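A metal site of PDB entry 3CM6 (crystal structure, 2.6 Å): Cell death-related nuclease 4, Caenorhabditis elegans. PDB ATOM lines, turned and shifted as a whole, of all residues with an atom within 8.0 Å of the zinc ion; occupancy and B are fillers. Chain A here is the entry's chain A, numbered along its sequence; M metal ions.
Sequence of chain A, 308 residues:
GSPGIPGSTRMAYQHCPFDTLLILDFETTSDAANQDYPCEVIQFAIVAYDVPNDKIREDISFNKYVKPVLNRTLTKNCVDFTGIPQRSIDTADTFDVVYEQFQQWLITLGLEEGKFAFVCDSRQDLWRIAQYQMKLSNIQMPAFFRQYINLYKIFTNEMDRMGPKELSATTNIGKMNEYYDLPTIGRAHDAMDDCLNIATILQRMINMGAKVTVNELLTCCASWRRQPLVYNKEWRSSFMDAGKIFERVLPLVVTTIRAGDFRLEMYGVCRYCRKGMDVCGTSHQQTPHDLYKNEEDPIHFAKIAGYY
SG of Cys 270 lies close to N of Tyr 272 (3.5 Å). The side-chain sulfur of Cys 270 sits close to the side-chain hydroxyl of Thr 219 (3.6 Å). N of Cys 270 lies within hydrogen-bond range of O of Lys 275 (3.0 Å). SG of Cys 273 sits close to N of Lys 275 (3.6 Å). The backbone carbonyl oxygen (O) of Cys 280 lies within hydrogen-bond range of the guanidinium group (NH1) of Arg 146 (3.4 Å).
Of the 19 residues printed, 4 come within 4 Å of the zinc ion.
The side-chain sulfur (SG) of Cys 220 is bound to the zinc ion, 2.3 Å away. SG of Cys 270 is bound to the zinc ion, at 2.4 Å. The zinc ion is bound by SG of Cys 273 (2.4 Å). SG of Cys 280 is bound to the zinc ion, at 2.4 Å.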
ATOM      1  N   ARG A 146      -9.633  15.879  12.923  1.00  0.00           N
ATOM      2  CA  ARG A 146     -10.126  14.616  13.476  1.00  0.00           C
ATOM      3  C   ARG A 146     -11.242  14.760  14.513  1.00  0.00           C
ATOM      4  O   ARG A 146     -11.719  13.770  15.067  1.00  0.00           O
ATOM      5  CB  ARG A 146      -8.968  13.755  14.002  1.00  0.00           C
ATOM      6  CG  ARG A 146      -7.969  13.330  12.901  1.00  0.00           C
ATOM      7  CD  ARG A 146      -6.880  12.442  13.446  1.00  0.00           C
ATOM      8  NE  ARG A 146      -7.440  11.224  14.025  1.00  0.00           N
ATOM      9  CZ  ARG A 146      -6.737  10.146  14.356  1.00  0.00           C
ATOM     10  NH1 ARG A 146      -5.427  10.103  14.165  1.00  0.00           N
ATOM     11  NH2 ARG A 146      -7.361   9.107  14.891  1.00  0.00           N
ATOM     12  N   LEU A 218     -12.670  11.252  14.194  1.00  0.00           N
ATOM     13  CA  LEU A 218     -11.960  10.377  13.270  1.00  0.00           C
ATOM     14  C   LEU A 218     -11.016   9.448  13.996  1.00  0.00           C
ATOM     15  O   LEU A 218     -10.125   9.869  14.732  1.00  0.00           O
ATOM     16  CB  LEU A 218     -11.239  11.152  12.178  1.00  0.00           C
ATOM     17  CG  LEU A 218     -12.142  11.928  11.216  1.00  0.00           C
ATOM     18  CD1 LEU A 218     -11.275  12.471  10.094  1.00  0.00           C
ATOM     19  CD2 LEU A 218     -13.251  11.056  10.681  1.00  0.00           C
ATOM     20  N   THR A 219     -11.213   8.159  13.739  1.00  0.00           N
ATOM     21  CA  THR A 219     -10.704   7.112  14.587  1.00  0.00           C
ATOM     22  C   THR A 219      -9.981   6.027  13.765  1.00  0.00           C
ATOM     23  O   THR A 219     -10.385   5.747  12.622  1.00  0.00           O
ATOM     24  CB  THR A 219     -11.900   6.546  15.401  1.00  0.00           C
ATOM     25  OG1 THR A 219     -11.675   6.768  16.792  1.00  0.00           O
ATOM     26  CG2 THR A 219     -12.165   5.104  15.129  1.00  0.00           C
ATOM     27  N   CYS A 220      -8.942   5.427  14.346  1.00  0.00           N
ATOM     28  CA  CYS A 220      -8.111   4.426  13.652  1.00  0.00           C
ATOM     29  C   CYS A 220      -8.822   3.120  13.413  1.00  0.00           C
ATOM     30  O   CYS A 220      -8.419   2.323  12.549  1.00  0.00           O
ATOM     31  CB  CYS A 220      -6.839   4.121  14.448  1.00  0.00           C
ATOM     32  SG  CYS A 220      -7.148   3.578  16.156  1.00  0.00           S
ATOM     33  N   CYS A 221      -9.894   2.882  14.150  1.00  0.00           N
ATOM     34  CA  CYS A 221     -10.371   1.535  14.292  1.00  0.00           C
ATOM     35  C   CYS A 221     -11.851   1.437  14.654  1.00  0.00           C
ATOM     36  O   CYS A 221     -12.358   2.196  15.491  1.00  0.00           O
ATOM     37  CB  CYS A 221      -9.526   0.851  15.339  1.00  0.00           C
ATOM     38  SG  CYS A 221      -9.395  -0.900  15.134  1.00  0.00           S
ATOM     39  N   LEU A 252      -8.665   6.270   8.667  1.00  0.00           N
ATOM     40  CA  LEU A 252      -9.497   6.808   9.732  1.00  0.00           C
ATOM     41  C   LEU A 252     -10.955   6.660   9.406  1.00  0.00           C
ATOM     42  O   LEU A 252     -11.376   6.892   8.273  1.00  0.00           O
ATOM     43  CB  LEU A 252      -9.162   8.279  10.036  1.00  0.00           C
ATOM     44  CG  LEU A 252      -7.690   8.643  10.214  1.00  0.00           C
ATOM     45  CD1 LEU A 252      -7.511  10.152  10.396  1.00  0.00           C
ATOM     46  CD2 LEU A 252      -7.019   7.855  11.338  1.00  0.00           C
ATOM     47  N   VAL A 269      -6.819  13.249  21.182  1.00  0.00           N
ATOM     48  CA  VAL A 269      -6.588  11.854  21.531  1.00  0.00           C
ATOM     49  C   VAL A 269      -7.626  11.043  20.777  1.00  0.00           C
ATOM     50  O   VAL A 269      -8.795  11.443  20.693  1.00  0.00           O
ATOM     51  CB  VAL A 269      -6.620  11.563  23.089  1.00  0.00           C
ATOM     52  CG1 VAL A 269      -6.289  12.824  23.899  1.00  0.00           C
ATOM     53  CG2 VAL A 269      -7.952  10.959  23.558  1.00  0.00           C
ATOM     54  N   CYS A 270      -7.194   9.925  20.216  1.00  0.00           N
ATOM     55  CA  CYS A 270      -8.066   9.093  19.420  1.00  0.00           C
ATOM     56  C   CYS A 270      -9.069   8.394  20.324  1.00  0.00           C
ATOM     57  O   CYS A 270      -8.694   7.826  21.353  1.00  0.00           O
ATOM     58  CB  CYS A 270      -7.253   8.084  18.603  1.00  0.00           C
ATOM     59  SG  CYS A 270      -8.209   6.755  17.804  1.00  0.00           S
ATOM     60  N   ARG A 271     -10.351   8.465  19.956  1.00  0.00           N
ATOM     61  CA  ARG A 271     -11.410   7.797  20.718  1.00  0.00           C
ATOM     62  C   ARG A 271     -11.246   6.296  20.887  1.00  0.00           C
ATOM     63  O   ARG A 271     -11.466   5.774  21.979  1.00  0.00           O
ATOM     64  CB  ARG A 271     -12.783   8.084  20.102  1.00  0.00           C
ATOM     65  CG  ARG A 271     -13.688   8.988  20.935  1.00  0.00           C
ATOM     66  CD  ARG A 271     -14.301   8.276  22.148  1.00  0.00           C
ATOM     67  NE  ARG A 271     -13.376   8.111  23.297  1.00  0.00           N
ATOM     68  CZ  ARG A 271     -12.986   9.069  24.144  1.00  0.00           C
ATOM     69  NH1 ARG A 271     -13.414  10.328  23.998  1.00  0.00           N
ATOM     70  NH2 ARG A 271     -12.151   8.783  25.146  1.00  0.00           N
ATOM     71  N   TYR A 272     -10.884   5.585  19.817  1.00  0.00           N
ATOM     72  CA  TYR A 272     -10.748   4.125  19.897  1.00  0.00           C
ATOM     73  C   TYR A 272      -9.658   3.654  20.840  1.00  0.00           C
ATOM     74  O   TYR A 272      -9.945   2.966  21.817  1.00  0.00           O
ATOM     75  CB  TYR A 272     -10.493   3.499  18.520  1.00  0.00           C
ATOM     76  CG  TYR A 272     -10.458   1.991  18.558  1.00  0.00           C
ATOM     77  CD1 TYR A 272     -11.637   1.263  18.498  1.00  0.00           C
ATOM     78  CD2 TYR A 272      -9.257   1.291  18.661  1.00  0.00           C
ATOM     79  CE1 TYR A 272     -11.638  -0.122  18.510  1.00  0.00           C
ATOM     80  CE2 TYR A 272      -9.219  -0.104  18.685  1.00  0.00           C
ATOM     81  CZ  TYR A 272     -10.418  -0.807  18.608  1.00  0.00           C
ATOM     82  OH  TYR A 272     -10.445  -2.177  18.623  1.00  0.00           O
ATOM     83  N   CYS A 273      -8.417   4.044  20.538  1.00  0.00           N
ATOM     84  CA  CYS A 273      -7.223   3.496  21.182  1.00  0.00           C
ATOM     85  C   CYS A 273      -6.689   4.357  22.312  1.00  0.00           C
ATOM     86  O   CYS A 273      -5.758   3.940  23.006  1.00  0.00           O
ATOM     87  CB  CYS A 273      -6.122   3.266  20.150  1.00  0.00           C
ATOM     88  SG  CYS A 273      -5.368   4.779  19.524  1.00  0.00           S
ATOM     89  N   ARG A 274      -7.234   5.566  22.479  1.00  0.00           N
ATOM     90  CA  ARG A 274      -6.845   6.492  23.575  1.00  0.00           C
ATOM     91  C   ARG A 274      -5.425   7.090  23.460  1.00  0.00           C
ATOM     92  O   ARG A 274      -4.958   7.740  24.397  1.00  0.00           O
ATOM     93  CB  ARG A 274      -6.998   5.822  24.955  1.00  0.00           C
ATOM     94  CG  ARG A 274      -8.309   5.081  25.199  1.00  0.00           C
ATOM     95  CD  ARG A 274      -9.342   5.957  25.881  1.00  0.00           C
ATOM     96  NE  ARG A 274     -10.210   5.156  26.746  1.00  0.00           N
ATOM     97  CZ  ARG A 274     -11.505   4.941  26.541  1.00  0.00           C
ATOM     98  NH1 ARG A 274     -12.108   5.470  25.476  1.00  0.00           N
ATOM     99  NH2 ARG A 274     -12.191   4.207  27.395  1.00  0.00           N
ATOM    100  N   LYS A 275      -4.744   6.872  22.345  1.00  0.00           N
ATOM    101  CA  LYS A 275      -3.395   7.408  22.171  1.00  0.00           C
ATOM    102  C   LYS A 275      -3.398   8.800  21.553  1.00  0.00           C
ATOM    103  O   LYS A 275      -4.425   9.261  21.046  1.00  0.00           O
ATOM    104  CB  LYS A 275      -2.563   6.473  21.285  1.00  0.00           C
ATOM    105  CG  LYS A 275      -2.215   5.139  21.913  1.00  0.00           C
ATOM    106  CD  LYS A 275      -1.123   4.479  21.074  1.00  0.00           C
ATOM    107  CE  LYS A 275      -0.764   3.093  21.604  1.00  0.00           C
ATOM    108  NZ  LYS A 275       0.293   2.465  20.746  1.00  0.00           N
ATOM    109  N   GLY A 276      -2.245   9.459  21.610  1.00  0.00           N
ATOM    110  CA  GLY A 276      -2.056  10.754  20.960  1.00  0.00           C
ATOM    111  C   GLY A 276      -2.153  10.581  19.450  1.00  0.00           C
ATOM    112  O   GLY A 276      -1.853   9.502  18.915  1.00  0.00           O
ATOM    113  N   MET A 277      -2.571  11.647  18.771  1.00  0.00           N
ATOM    114  CA  MET A 277      -2.866  11.549  17.328  1.00  0.00           C
ATOM    115  C   MET A 277      -1.660  11.878  16.458  1.00  0.00           C
ATOM    116  O   MET A 277      -1.806  12.220  15.261  1.00  0.00           O
ATOM    117  CB  MET A 277      -4.022  12.468  16.952  1.00  0.00           C
ATOM    118  CG  MET A 277      -5.365  11.953  17.383  1.00  0.00           C
ATOM    119  SD  MET A 277      -6.585  13.216  16.977  1.00  0.00           S
ATOM    120  CE  MET A 277      -8.112  12.357  17.471  1.00  0.00           C
ATOM    121  N   VAL A 279       0.999   9.532  17.272  1.00  0.00           N
ATOM    122  CA  VAL A 279       1.183   8.061  17.279  1.00  0.00           C
ATOM    123  C   VAL A 279       0.139   7.387  16.360  1.00  0.00           C
ATOM    124  O   VAL A 279       0.442   7.101  15.174  1.00  0.00           O
ATOM    125  CB  VAL A 279       1.100   7.473  18.704  1.00  0.00           C
ATOM    126  CG1 VAL A 279       1.561   6.011  18.719  1.00  0.00           C
ATOM    127  CG2 VAL A 279       1.923   8.288  19.679  1.00  0.00           C
ATOM    128  N   CYS A 280      -1.069   7.149  16.893  1.00  0.00           N
ATOM    129  CA  CYS A 280      -2.228   6.718  16.079  1.00  0.00           C
ATOM    130  C   CYS A 280      -2.419   7.669  14.903  1.00  0.00           C
ATOM    131  O   CYS A 280      -2.411   8.907  15.071  1.00  0.00           O
ATOM    132  CB  CYS A 280      -3.512   6.668  16.931  1.00  0.00           C
ATOM    133  SG  CYS A 280      -5.066   6.854  15.991  1.00  0.00           S
ATOM    134  N   GLY A 281      -2.579   7.099  13.721  1.00  0.00           N
ATOM    135  CA  GLY A 281      -2.667   7.920  12.523  1.00  0.00           C
ATOM    136  C   GLY A 281      -1.660   7.561  11.451  1.00  0.00           C
ATOM    137  O   GLY A 281      -1.991   7.639  10.274  1.00  0.00           O
ATOM    138  N   GLN A 285      -4.648   0.745  10.460  1.00  0.00           N
ATOM    139  CA  GLN A 285      -4.772  -0.378  11.403  1.00  0.00           C
ATOM    140  C   GLN A 285      -5.697  -1.511  10.943  1.00  0.00           C
ATOM    141  O   GLN A 285      -5.836  -2.512  11.641  1.00  0.00           O
ATOM    142  CB  GLN A 285      -5.254   0.128  12.786  1.00  0.00           C
ATOM    143  CG  GLN A 285      -4.441   1.257  13.381  1.00  0.00           C
ATOM    144  CD  GLN A 285      -3.028   0.856  13.689  1.00  0.00           C
ATOM    145  OE1 GLN A 285      -2.089   1.526  13.283  1.00  0.00           O
ATOM    146  NE2 GLN A 285      -2.865  -0.242  14.413  1.00  0.00           N
HETATM  147 ZN    ZN M   1      -6.337   5.329  17.384  1.00  0.00          ZN
